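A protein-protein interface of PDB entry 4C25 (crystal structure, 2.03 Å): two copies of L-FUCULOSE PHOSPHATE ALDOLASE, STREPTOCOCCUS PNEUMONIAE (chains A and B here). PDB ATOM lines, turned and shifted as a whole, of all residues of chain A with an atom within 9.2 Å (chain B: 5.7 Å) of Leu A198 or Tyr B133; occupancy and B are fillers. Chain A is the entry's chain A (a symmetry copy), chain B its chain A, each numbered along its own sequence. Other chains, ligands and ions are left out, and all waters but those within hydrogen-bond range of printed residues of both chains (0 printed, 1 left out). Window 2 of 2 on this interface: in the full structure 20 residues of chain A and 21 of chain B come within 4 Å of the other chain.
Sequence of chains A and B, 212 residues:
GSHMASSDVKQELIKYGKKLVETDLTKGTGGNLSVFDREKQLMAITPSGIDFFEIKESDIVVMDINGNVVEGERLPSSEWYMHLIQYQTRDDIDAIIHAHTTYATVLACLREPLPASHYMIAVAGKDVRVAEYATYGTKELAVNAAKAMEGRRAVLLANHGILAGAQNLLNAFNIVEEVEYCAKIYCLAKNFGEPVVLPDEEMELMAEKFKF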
ATOM      1  N   PRO A 115      -7.346 -16.151   5.135  1.00  0.00           N
ATOM      2  CA  PRO A 115      -8.127 -15.593   4.007  1.00  0.00           C
ATOM      3  C   PRO A 115      -8.797 -16.697   3.170  1.00  0.00           C
ATOM      4  O   PRO A 115      -8.704 -17.877   3.528  1.00  0.00           O
ATOM      5  CB  PRO A 115      -7.072 -14.828   3.191  1.00  0.00           C
ATOM      6  CG  PRO A 115      -5.832 -15.615   3.407  1.00  0.00           C
ATOM      7  CD  PRO A 115      -5.909 -16.205   4.803  1.00  0.00           C
ATOM      8  N   ALA A 116      -9.467 -16.322   2.074  1.00  0.00           N
ATOM      9  CA  ALA A 116     -10.283 -17.272   1.300  1.00  0.00           C
ATOM     10  C   ALA A 116      -9.593 -17.862   0.058  1.00  0.00           C
ATOM     11  O   ALA A 116     -10.068 -17.741  -1.090  1.00  0.00           O
ATOM     12  CB  ALA A 116     -11.625 -16.657   0.959  1.00  0.00           C
ATOM     13  N   SER A 117      -8.451 -18.490   0.318  1.00  0.00           N
ATOM     14  CA  SER A 117      -7.771 -19.342  -0.639  1.00  0.00           C
ATOM     15  C   SER A 117      -8.614 -20.587  -0.916  1.00  0.00           C
ATOM     16  O   SER A 117      -8.544 -21.124  -2.010  1.00  0.00           O
ATOM     17  CB  SER A 117      -6.375 -19.727  -0.128  1.00  0.00           C
ATOM     18  OG  SER A 117      -6.428 -20.108   1.256  1.00  0.00           O
ATOM     19  N   HIS A 118      -9.410 -21.041   0.051  1.00  0.00           N
ATOM     20  CA  HIS A 118     -10.418 -22.089  -0.222  1.00  0.00           C
ATOM     21  C   HIS A 118     -11.822 -21.595   0.116  1.00  0.00           C
ATOM     22  O   HIS A 118     -12.050 -20.978   1.157  1.00  0.00           O
ATOM     23  CB  HIS A 118     -10.136 -23.372   0.563  1.00  0.00           C
ATOM     24  CG  HIS A 118     -10.836 -24.577   0.005  1.00  0.00           C
ATOM     25  ND1 HIS A 118     -12.174 -24.816   0.206  1.00  0.00           N
ATOM     26  CD2 HIS A 118     -10.385 -25.593  -0.774  1.00  0.00           C
ATOM     27  CE1 HIS A 118     -12.521 -25.937  -0.405  1.00  0.00           C
ATOM     28  NE2 HIS A 118     -11.453 -26.432  -1.007  1.00  0.00           N
ATOM     29  N   TYR A 119     -12.766 -21.873  -0.770  1.00  0.00           N
ATOM     30  CA  TYR A 119     -14.105 -21.314  -0.664  1.00  0.00           C
ATOM     31  C   TYR A 119     -14.857 -21.811   0.578  1.00  0.00           C
ATOM     32  O   TYR A 119     -15.730 -21.101   1.075  1.00  0.00           O
ATOM     33  CB  TYR A 119     -14.927 -21.551  -1.965  1.00  0.00           C
ATOM     34  CG  TYR A 119     -15.611 -22.912  -2.065  1.00  0.00           C
ATOM     35  CD1 TYR A 119     -16.854 -23.168  -1.444  1.00  0.00           C
ATOM     36  CD2 TYR A 119     -15.020 -23.948  -2.777  1.00  0.00           C
ATOM     37  CE1 TYR A 119     -17.474 -24.428  -1.537  1.00  0.00           C
ATOM     38  CE2 TYR A 119     -15.635 -25.197  -2.873  1.00  0.00           C
ATOM     39  CZ  TYR A 119     -16.847 -25.432  -2.253  1.00  0.00           C
ATOM     40  OH  TYR A 119     -17.403 -26.702  -2.393  1.00  0.00           O
ATOM     41  N   MET A 120     -14.545 -23.014   1.076  1.00  0.00           N
ATOM     42  CA  MET A 120     -15.322 -23.580   2.208  1.00  0.00           C
ATOM     43  C   MET A 120     -15.239 -22.765   3.528  1.00  0.00           C
ATOM     44  O   MET A 120     -15.987 -23.014   4.480  1.00  0.00           O
ATOM     45  CB  MET A 120     -14.937 -25.036   2.466  1.00  0.00           C
ATOM     46  CG  MET A 120     -15.535 -26.050   1.497  1.00  0.00           C
ATOM     47  SD  MET A 120     -17.345 -26.224   1.503  1.00  0.00           S
ATOM     48  CE  MET A 120     -17.742 -26.135   3.246  1.00  0.00           C
ATOM     49  N   ILE A 121     -14.315 -21.804   3.564  1.00  0.00           N
ATOM     50  CA  ILE A 121     -14.133 -20.861   4.664  1.00  0.00           C
ATOM     51  C   ILE A 121     -15.447 -20.135   4.927  1.00  0.00           C
ATOM     52  O   ILE A 121     -15.724 -19.685   6.047  1.00  0.00           O
ATOM     53  CB  ILE A 121     -12.998 -19.838   4.344  1.00  0.00           C
ATOM     54  CG1 ILE A 121     -12.545 -19.091   5.603  1.00  0.00           C
ATOM     55  CG2 ILE A 121     -13.450 -18.787   3.361  1.00  0.00           C
ATOM     56  CD1 ILE A 121     -12.381 -19.987   6.825  1.00  0.00           C
ATOM     57  N   ALA A 122     -16.263 -20.031   3.880  1.00  0.00           N
ATOM     58  CA  ALA A 122     -17.579 -19.424   3.986  1.00  0.00           C
ATOM     59  C   ALA A 122     -18.472 -20.005   5.064  1.00  0.00           C
ATOM     60  O   ALA A 122     -19.378 -19.310   5.503  1.00  0.00           O
ATOM     61  CB  ALA A 122     -18.299 -19.402   2.643  1.00  0.00           C
ATOM     62  N   GLY A 125     -16.992 -17.233   7.501  1.00  0.00           N
ATOM     63  CA  GLY A 125     -16.985 -15.861   7.004  1.00  0.00           C
ATOM     64  C   GLY A 125     -16.144 -15.768   5.753  1.00  0.00           C
ATOM     65  O   GLY A 125     -15.827 -16.785   5.154  1.00  0.00           O
ATOM     66  N   LYS A 126     -15.773 -14.559   5.361  1.00  0.00           N
ATOM     67  CA  LYS A 126     -14.865 -14.394   4.221  1.00  0.00           C
ATOM     68  C   LYS A 126     -13.422 -14.657   4.643  1.00  0.00           C
ATOM     69  O   LYS A 126     -12.550 -14.959   3.809  1.00  0.00           O
ATOM     70  CB  LYS A 126     -14.981 -12.984   3.625  1.00  0.00           C
ATOM     71  CG  LYS A 126     -14.555 -11.880   4.570  1.00  0.00           C
ATOM     72  CD  LYS A 126     -14.693 -10.534   3.895  1.00  0.00           C
ATOM     73  CE  LYS A 126     -13.609  -9.573   4.363  1.00  0.00           C
ATOM     74  NZ  LYS A 126     -13.809  -8.245   3.713  1.00  0.00           N
ATOM     75  N   ASP A 127     -13.176 -14.482   5.940  1.00  0.00           N
ATOM     76  CA  ASP A 127     -11.907 -14.780   6.561  1.00  0.00           C
ATOM     77  C   ASP A 127     -12.094 -15.085   8.040  1.00  0.00           C
ATOM     78  O   ASP A 127     -13.144 -14.778   8.634  1.00  0.00           O
ATOM     79  CB  ASP A 127     -10.885 -13.641   6.354  1.00  0.00           C
ATOM     80  CG  ASP A 127     -11.421 -12.282   6.725  1.00  0.00           C
ATOM     81  OD1 ASP A 127     -12.289 -12.191   7.610  1.00  0.00           O
ATOM     82  OD2 ASP A 127     -10.972 -11.291   6.118  1.00  0.00           O
ATOM     83  N   PRO A 195      -0.702 -18.435  -2.424  1.00  0.00           N
ATOM     84  CA  PRO A 195      -2.093 -18.909  -2.524  1.00  0.00           C
ATOM     85  C   PRO A 195      -3.008 -17.831  -3.156  1.00  0.00           C
ATOM     86  O   PRO A 195      -2.869 -16.652  -2.845  1.00  0.00           O
ATOM     87  CB  PRO A 195      -2.491 -19.170  -1.062  1.00  0.00           C
ATOM     88  CG  PRO A 195      -1.223 -19.245  -0.299  1.00  0.00           C
ATOM     89  CD  PRO A 195      -0.225 -18.390  -1.028  1.00  0.00           C
ATOM     90  N   VAL A 196      -3.902 -18.236  -4.065  1.00  0.00           N
ATOM     91  CA  VAL A 196      -4.862 -17.311  -4.698  1.00  0.00           C
ATOM     92  C   VAL A 196      -6.095 -17.156  -3.791  1.00  0.00           C
ATOM     93  O   VAL A 196      -6.816 -18.144  -3.486  1.00  0.00           O
ATOM     94  CB  VAL A 196      -5.273 -17.795  -6.124  1.00  0.00           C
ATOM     95  CG1 VAL A 196      -6.243 -16.817  -6.779  1.00  0.00           C
ATOM     96  CG2 VAL A 196      -4.038 -18.000  -6.995  1.00  0.00           C
ATOM     97  N   VAL A 197      -6.326 -15.923  -3.347  1.00  0.00           N
ATOM     98  CA  VAL A 197      -7.445 -15.614  -2.440  1.00  0.00           C
ATOM     99  C   VAL A 197      -8.652 -15.160  -3.266  1.00  0.00           C
ATOM    100  O   VAL A 197      -8.551 -14.204  -4.078  1.00  0.00           O
ATOM    101  CB  VAL A 197      -7.035 -14.568  -1.365  1.00  0.00           C
ATOM    102  CG1 VAL A 197      -8.251 -14.043  -0.607  1.00  0.00           C
ATOM    103  CG2 VAL A 197      -6.001 -15.160  -0.383  1.00  0.00           C
ATOM    104  N   LEU A 198      -9.788 -15.841  -3.076  1.00  0.00           N
ATOM    105  CA  LEU A 198     -11.018 -15.471  -3.767  1.00  0.00           C
ATOM    106  C   LEU A 198     -11.435 -14.073  -3.310  1.00  0.00           C
ATOM    107  O   LEU A 198     -11.289 -13.758  -2.144  1.00  0.00           O
ATOM    108  CB  LEU A 198     -12.153 -16.492  -3.512  1.00  0.00           C
ATOM    109  CG  LEU A 198     -11.882 -17.944  -3.893  1.00  0.00           C
ATOM    110  CD1 LEU A 198     -12.952 -18.873  -3.332  1.00  0.00           C
ATOM    111  CD2 LEU A 198     -11.742 -18.097  -5.402  1.00  0.00           C
ATOM    112  N   PRO A 199     -11.938 -13.229  -4.237  1.00  0.00           N
ATOM    113  CA  PRO A 199     -12.324 -11.854  -3.829  1.00  0.00           C
ATOM    114  C   PRO A 199     -13.597 -11.785  -2.960  1.00  0.00           C
ATOM    115  O   PRO A 199     -14.401 -12.741  -2.913  1.00  0.00           O
ATOM    116  CB  PRO A 199     -12.521 -11.120  -5.164  1.00  0.00           C
ATOM    117  CG  PRO A 199     -12.758 -12.193  -6.183  1.00  0.00           C
ATOM    118  CD  PRO A 199     -12.062 -13.446  -5.697  1.00  0.00           C
ATOM    119  N   ASP A 200     -13.751 -10.658  -2.267  1.00  0.00           N
ATOM    120  CA  ASP A 200     -14.913 -10.406  -1.390  1.00  0.00           C
ATOM    121  C   ASP A 200     -16.263 -10.608  -2.066  1.00  0.00           C
ATOM    122  O   ASP A 200     -17.171 -11.215  -1.478  1.00  0.00           O
ATOM    123  CB  ASP A 200     -14.851  -8.979  -0.827  1.00  0.00           C
ATOM    124  CG  ASP A 200     -13.856  -8.838   0.297  1.00  0.00           C
ATOM    125  OD1 ASP A 200     -13.040  -9.776   0.509  1.00  0.00           O
ATOM    126  OD2 ASP A 200     -13.900  -7.787   0.975  1.00  0.00           O
ATOM    127  N   GLU A 201     -16.409 -10.092  -3.288  1.00  0.00           N
ATOM    128  CA  GLU A 201     -17.663 -10.287  -4.012  1.00  0.00           C
ATOM    129  C   GLU A 201     -18.021 -11.790  -4.145  1.00  0.00           C
ATOM    130  O   GLU A 201     -19.153 -12.192  -3.847  1.00  0.00           O
ATOM    131  CB  GLU A 201     -17.636  -9.605  -5.377  1.00  0.00           C
ATOM    132  CG  GLU A 201     -19.021  -9.501  -6.007  1.00  0.00           C
ATOM    133  CD  GLU A 201     -19.010  -8.816  -7.360  1.00  0.00           C
ATOM    134  OE1 GLU A 201     -18.421  -7.716  -7.492  1.00  0.00           O
ATOM    135  OE2 GLU A 201     -19.600  -9.379  -8.300  1.00  0.00           O
ATOM    136  N   GLU A 202     -17.054 -12.613  -4.553  1.00  0.00           N
ATOM    137  CA  GLU A 202     -17.294 -14.057  -4.639  1.00  0.00           C
ATOM    138  C   GLU A 202     -17.614 -14.615  -3.244  1.00  0.00           C
ATOM    139  O   GLU A 202     -18.562 -15.363  -3.080  1.00  0.00           O
ATOM    140  CB  GLU A 202     -16.121 -14.790  -5.321  1.00  0.00           C
ATOM    141  CG  GLU A 202     -16.274 -16.315  -5.454  1.00  0.00           C
ATOM    142  CD  GLU A 202     -17.245 -16.763  -6.546  1.00  0.00           C
ATOM    143  OE1 GLU A 202     -17.684 -15.917  -7.345  1.00  0.00           O
ATOM    144  OE2 GLU A 202     -17.575 -17.970  -6.626  1.00  0.00           O
ATOM    145  N   MET A 203     -16.870 -14.201  -2.223  1.00  0.00           N
ATOM    146  CA  MET A 203     -17.168 -14.690  -0.871  1.00  0.00           C
ATOM    147  C   MET A 203     -18.566 -14.294  -0.379  1.00  0.00           C
ATOM    148  O   MET A 203     -19.267 -15.088   0.279  1.00  0.00           O
ATOM    149  CB  MET A 203     -16.045 -14.300   0.110  1.00  0.00           C
ATOM    150  CG  MET A 203     -14.728 -15.025  -0.182  1.00  0.00           C
ATOM    151  SD  MET A 203     -14.978 -16.783  -0.564  1.00  0.00           S
ATOM    152  CE  MET A 203     -15.594 -17.444   0.981  1.00  0.00           C
ATOM    153  N   GLU A 204     -18.974 -13.072  -0.715  1.00  0.00           N
ATOM    154  CA  GLU A 204     -20.365 -12.611  -0.496  1.00  0.00           C
ATOM    155  C   GLU A 204     -21.398 -13.556  -1.108  1.00  0.00           C
ATOM    156  O   GLU A 204     -22.356 -13.999  -0.442  1.00  0.00           O
ATOM    157  CB  GLU A 204     -20.532 -11.220  -1.086  1.00  0.00           C
ATOM    158  CG  GLU A 204     -21.664 -10.401  -0.509  1.00  0.00           C
ATOM    159  CD  GLU A 204     -21.456  -8.917  -0.768  1.00  0.00           C
ATOM    160  OE1 GLU A 204     -20.969  -8.563  -1.871  1.00  0.00           O
ATOM    161  OE2 GLU A 204     -21.749  -8.101   0.140  1.00  0.00           O
ATOM    162  N   LEU A 205     -21.190 -13.862  -2.391  1.00  0.00           N
ATOM    163  CA  LEU A 205     -22.007 -14.840  -3.091  1.00  0.00           C
ATOM    164  C   LEU A 205     -21.967 -16.171  -2.338  1.00  0.00           C
ATOM    165  O   LEU A 205     -23.018 -16.792  -2.105  1.00  0.00           O
ATOM    166  CB  LEU A 205     -21.505 -14.979  -4.533  1.00  0.00           C
ATOM    167  CG  LEU A 205     -21.803 -16.133  -5.512  1.00  0.00           C
ATOM    168  CD1 LEU A 205     -23.254 -16.611  -5.513  1.00  0.00           C
ATOM    169  CD2 LEU A 205     -21.359 -15.697  -6.916  1.00  0.00           C
ATOM    170  N   MET A 206     -20.757 -16.592  -1.935  1.00  0.00           N
ATOM    171  CA  MET A 206     -20.606 -17.867  -1.250  1.00  0.00           C
ATOM    172  C   MET A 206     -21.480 -17.936  -0.008  1.00  0.00           C
ATOM    173  O   MET A 206     -22.232 -18.906   0.167  1.00  0.00           O
ATOM    174  CB  MET A 206     -19.144 -18.158  -0.931  1.00  0.00           C
ATOM    175  CG  MET A 206     -18.761 -19.616  -1.142  1.00  0.00           C
ATOM    176  SD  MET A 206     -18.848 -20.164  -2.869  1.00  0.00           S
ATOM    177  CE  MET A 206     -17.607 -19.087  -3.609  1.00  0.00           C
ATOM    178  N   LYS A 209     -25.046 -18.577  -0.952  1.00  0.00           N
ATOM    179  CA  LYS A 209     -25.305 -19.967  -1.385  1.00  0.00           C
ATOM    180  C   LYS A 209     -25.367 -20.940  -0.220  1.00  0.00           C
ATOM    181  O   LYS A 209     -26.191 -21.860  -0.216  1.00  0.00           O
ATOM    182  CB  LYS A 209     -24.277 -20.451  -2.409  1.00  0.00           C
ATOM    183  CG  LYS A 209     -24.335 -19.697  -3.736  1.00  0.00           C
ATOM    184  CD  LYS A 209     -23.708 -20.489  -4.864  1.00  0.00           C
ATOM    185  CE  LYS A 209     -24.615 -21.614  -5.329  1.00  0.00           C
ATOM    186  NZ  LYS A 209     -24.228 -22.063  -6.704  1.00  0.00           N
ATOM    187  N   PHE A 210     -24.497 -20.717   0.766  1.00  0.00           N
ATOM    188  CA  PHE A 210     -24.432 -21.558   1.963  1.00  0.00           C
ATOM    189  C   PHE A 210     -25.682 -21.445   2.837  1.00  0.00           C
ATOM    190  O   PHE A 210     -26.044 -22.415   3.509  1.00  0.00           O
ATOM    191  CB  PHE A 210     -23.164 -21.254   2.774  1.00  0.00           C
ATOM    192  CG  PHE A 210     -21.925 -21.933   2.250  1.00  0.00           C
ATOM    193  CD1 PHE A 210     -21.800 -22.258   0.893  1.00  0.00           C
ATOM    194  CD2 PHE A 210     -20.872 -22.234   3.107  1.00  0.00           C
ATOM    195  CE1 PHE A 210     -20.662 -22.886   0.410  1.00  0.00           C
ATOM    196  CE2 PHE A 210     -19.724 -22.846   2.624  1.00  0.00           C
ATOM    197  CZ  PHE A 210     -19.620 -23.180   1.274  1.00  0.00           C
ATOM    198  N   ARG B 111      -3.466 -22.610  -7.935  1.00  0.00           N
ATOM    199  CA  ARG B 111      -3.724 -22.749  -9.360  1.00  0.00           C
ATOM    200  C   ARG B 111      -2.425 -23.200 -10.079  1.00  0.00           C
ATOM    201  O   ARG B 111      -1.942 -22.553 -11.013  1.00  0.00           O
ATOM    202  CB  ARG B 111      -4.337 -21.440  -9.922  1.00  0.00           C
ATOM    203  CG  ARG B 111      -5.731 -21.168  -9.378  1.00  0.00           C
ATOM    204  CD  ARG B 111      -6.203 -19.759  -9.692  1.00  0.00           C
ATOM    205  NE  ARG B 111      -7.418 -19.445  -8.941  1.00  0.00           N
ATOM    206  CZ  ARG B 111      -8.255 -18.447  -9.206  1.00  0.00           C
ATOM    207  NH1 ARG B 111      -8.036 -17.623 -10.236  1.00  0.00           N
ATOM    208  NH2 ARG B 111      -9.317 -18.274  -8.433  1.00  0.00           N
ATOM    209  N   ALA B 131      -8.356 -26.605 -13.830  1.00  0.00           N
ATOM    210  CA  ALA B 131      -9.486 -25.871 -14.430  1.00  0.00           C
ATOM    211  C   ALA B 131      -9.479 -24.411 -13.992  1.00  0.00           C
ATOM    212  O   ALA B 131      -8.940 -24.089 -12.941  1.00  0.00           O
ATOM    213  CB  ALA B 131     -10.834 -26.515 -14.072  1.00  0.00           C
ATOM    214  N   GLU B 132     -10.061 -23.547 -14.824  1.00  0.00           N
ATOM    215  CA  GLU B 132     -10.291 -22.140 -14.504  1.00  0.00           C
ATOM    216  C   GLU B 132     -11.346 -22.049 -13.409  1.00  0.00           C
ATOM    217  O   GLU B 132     -12.277 -22.914 -13.359  1.00  0.00           O
ATOM    218  CB  GLU B 132     -10.785 -21.403 -15.749  1.00  0.00           C
ATOM    219  CG  GLU B 132      -9.796 -21.417 -16.908  1.00  0.00           C
ATOM    220  CD  GLU B 132     -10.124 -20.395 -17.991  1.00  0.00           C
ATOM    221  OE1 GLU B 132     -11.186 -20.524 -18.651  1.00  0.00           O
ATOM    222  OE2 GLU B 132      -9.314 -19.457 -18.181  1.00  0.00           O
ATOM    223  N   TYR B 133     -11.233 -21.019 -12.552  1.00  0.00           N
ATOM    224  CA  TYR B 133     -12.120 -20.929 -11.369  1.00  0.00           C
ATOM    225  C   TYR B 133     -13.596 -20.735 -11.724  1.00  0.00           C
ATOM    226  O   TYR B 133     -13.936 -19.953 -12.601  1.00  0.00           O
ATOM    227  CB  TYR B 133     -11.672 -19.889 -10.304  1.00  0.00           C
ATOM    228  CG  TYR B 133     -12.711 -19.779  -9.175  1.00  0.00           C
ATOM    229  CD1 TYR B 133     -12.743 -20.717  -8.157  1.00  0.00           C
ATOM    230  CD2 TYR B 133     -13.701 -18.791  -9.187  1.00  0.00           C
ATOM    231  CE1 TYR B 133     -13.711 -20.689  -7.163  1.00  0.00           C
ATOM    232  CE2 TYR B 133     -14.672 -18.744  -8.186  1.00  0.00           C
ATOM    233  CZ  TYR B 133     -14.679 -19.704  -7.181  1.00  0.00           C
ATOM    234  OH  TYR B 133     -15.617 -19.688  -6.149  1.00  0.00           O
ATOM    235  N   ALA B 134     -14.471 -21.455 -11.028  1.00  0.00           N
ATOM    236  CA  ALA B 134     -15.890 -21.129 -11.051  1.00  0.00           C
ATOM    237  C   ALA B 134     -16.532 -21.633  -9.793  1.00  0.00           C
ATOM    238  O   ALA B 134     -16.079 -22.648  -9.247  1.00  0.00           O
ATOM    239  CB  ALA B 134     -16.576 -21.723 -12.274  1.00  0.00           C
ATOM    240  N   THR B 135     -17.591 -20.935  -9.373  1.00  0.00           N
ATOM    241  CA  THR B 135     -18.363 -21.180  -8.152  1.00  0.00           C
ATOM    242  C   THR B 135     -18.852 -22.635  -8.110  1.00  0.00           C
ATOM    243  O   THR B 135     -19.318 -23.138  -9.103  1.00  0.00           O
ATOM    244  CB  THR B 135     -19.614 -20.224  -8.124  1.00  0.00           C
ATOM    245  OG1 THR B 135     -19.222 -18.876  -8.439  1.00  0.00           O
ATOM    246  CG2 THR B 135     -20.316 -20.235  -6.805  1.00  0.00           C
ATOM    247  N   TYR B 136     -18.724 -23.314  -6.976  1.00  0.00           N
ATOM    248  CA  TYR B 136     -19.192 -24.696  -6.902  1.00  0.00           C
ATOM    249  C   TYR B 136     -20.606 -24.748  -7.429  1.00  0.00           C
ATOM    250  O   TYR B 136     -21.333 -23.751  -7.326  1.00  0.00           O
ATOM    251  CB  TYR B 136     -19.165 -25.256  -5.481  1.00  0.00           C
ATOM    252  CG  TYR B 136     -20.325 -24.851  -4.592  1.00  0.00           C
ATOM    253  CD1 TYR B 136     -20.303 -23.637  -3.878  1.00  0.00           C
ATOM    254  CD2 TYR B 136     -21.438 -25.685  -4.443  1.00  0.00           C
ATOM    255  CE1 TYR B 136     -21.369 -23.269  -3.051  1.00  0.00           C
ATOM    256  CE2 TYR B 136     -22.508 -25.326  -3.632  1.00  0.00           C
ATOM    257  CZ  TYR B 136     -22.467 -24.115  -2.941  1.00  0.00           C
ATOM    258  OH  TYR B 136     -23.524 -23.773  -2.121  1.00  0.00           O
ATOM    259  N   LEU B 141     -18.426 -24.030 -13.867  1.00  0.00           N
ATOM    260  CA  LEU B 141     -17.529 -25.024 -13.242  1.00  0.00           C
ATOM    261  C   LEU B 141     -17.434 -26.301 -14.081  1.00  0.00           C
ATOM    262  O   LEU B 141     -16.324 -26.736 -14.432  1.00  0.00           O
ATOM    263  CB  LEU B 141     -17.970 -25.388 -11.802  1.00  0.00           C
ATOM    264  CG  LEU B 141     -16.951 -26.255 -11.042  1.00  0.00           C
ATOM    265  CD1 LEU B 141     -15.593 -25.549 -11.099  1.00  0.00           C
ATOM    266  CD2 LEU B 141     -17.378 -26.488  -9.598  1.00  0.00           C
ATOM    267  N   ASN B 144     -15.748 -25.679 -17.299  1.00  0.00           N
ATOM    268  CA  ASN B 144     -14.305 -25.499 -17.028  1.00  0.00           C
ATOM    269  C   ASN B 144     -13.620 -26.852 -16.725  1.00  0.00           C
ATOM    270  O   ASN B 144     -12.506 -27.109 -17.176  1.00  0.00           O
ATOM    271  CB  ASN B 144     -14.106 -24.498 -15.891  1.00  0.00           C
ATOM    272  CG  ASN B 144     -14.500 -23.058 -16.283  1.00  0.00           C
ATOM    273  OD1 ASN B 144     -14.791 -22.756 -17.455  1.00  0.00           O
ATOM    274  ND2 ASN B 144     -14.495 -22.163 -15.295  1.00  0.00           N
ATOM    275  N   ALA B 158      -9.797 -25.220  -9.335  1.00  0.00           N
ATOM    276  CA  ALA B 158      -9.167 -24.062  -8.728  1.00  0.00           C
ATOM    277  C   ALA B 158      -9.843 -23.742  -7.416  1.00  0.00           C
ATOM    278  O   ALA B 158     -11.054 -23.707  -7.341  1.00  0.00           O
ATOM    279  CB  ALA B 158      -9.248 -22.856  -9.676  1.00  0.00           C
ATOM    280  N   ASN B 159      -9.045 -23.561  -6.371  1.00  0.00           N
ATOM    281  CA  ASN B 159      -9.542 -23.187  -5.041  1.00  0.00           C
ATOM    282  C   ASN B 159     -10.627 -24.093  -4.535  1.00  0.00           C
ATOM    283  O   ASN B 159     -11.455 -23.618  -3.772  1.00  0.00           O
ATOM    284  CB  ASN B 159     -10.030 -21.737  -5.000  1.00  0.00           C
ATOM    285  CG  ASN B 159      -8.987 -20.760  -5.519  1.00  0.00           C
ATOM    286  OD1 ASN B 159      -8.182 -20.205  -4.751  1.00  0.00           O
ATOM    287  ND2 ASN B 159      -8.947 -20.597  -6.812  1.00  0.00           N
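Of the 25 printed residues of chain A, 9 touch a printed residue of chain B. Along chain A the printed residues that touch a printed residue of chain B span positions 117 to 210. Of the 11 printed residues of chain B, 5 touch a printed residue of chain A. Printed residues of chain B that touch a printed residue of chain A: Arg B111, Tyr B133, Thr B135, Tyr B136 and Asn B159. Hydrophobic or aromatic side chains of chain B that line the printed part of chain A: Tyr B133 and Tyr B136. Among the printed residues, 16 pairs touch across the chains. Among the printed residues, no Asp or Glu carboxylate lies within 4 Å of a Lys or Arg side-chain nitrogen of the other chain.
The side-chain carboxylate of Glu A202 is in hydrogen-bond range of the side-chain hydroxyl of Tyr B133 (2.6 Å). OG1 of Thr B135 is in hydrogen-bond range of OE2 of Glu A202. O of Tyr B136 lies within hydrogen-bond range of NZ of Lys A209 (3.4 Å). The side-chain amide oxygen of Asn B159 sits close to the backbone carbonyl oxygen of Ser A117, 2.9 Å away. The side-chain amide oxygen (OD1) of Asn B159 lies close to the backbone carbonyl oxygen (O) of Val A196, 2.8 Å away.
No position is printed for both chains. Of the 16 pairs that touch across the chains among the printed residues, none has its exchanged pair printed and touching as well.
The side-chain amide nitrogen of Asn B159 lies close to the guanidinium group of Arg B111, 2.9 Å away. The backbone carbonyl oxygen of Ala A116 sits at hydrogen-bond distance from the backbone NH of Leu A198, at 2.8 Å. ND1 of His A118 lies within hydrogen-bond range of N of Met A120 (3.1 Å).
Among the printed residues, merely in contact across the chains: His A118 with Asn B159 (3.7 Å), Tyr A119 with Tyr B136 (3.8 Å), Tyr A119 with Asn B159 (3.7 Å), Val A196 with Arg B111 (3.5 Å), Leu A198 with Arg B111 (3.9 Å), Leu A198 with Tyr B133 (3.7 Å), Leu A198 with Asn B159 (3.8 Å), Met A206 with Tyr B133 (3.3 Å), Met A206 with Tyr B136 (3.9 Å), Lys A209 with Thr B135 (3.9 Å) and Phe A210 with Tyr B136 (3.6 Å).
Of the printed residues of chain B, His A118 touches Asn B159. Of the printed residues of chain B, Val A196 touches Arg B111 (3.5 Å) and Asn B159 (2.8 Å). Printed residues of chain B within 4 Å of Leu A198: Arg B111, Tyr B133 and Asn B159. Printed residues of chain B within 4 Å of Lys A209: Thr B135 and Tyr B136. Of the printed residues of chain A, Arg B111 touches Val A196 and Leu A198. Tyr B133 touches three residues of chain A. Of the printed residues of chain A, Thr B135 touches Glu A202 (2.6 Å) and Lys A209 (3.9 Å). Ala B158 touches none of the printed residues of chain A. The nearest printed residue of chain B that does not touch Leu A198 is Ala B158 (6.0 Å). The nearest printed residue of chain B that does not touch Phe A210 is Thr B135 (7.7 Å).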
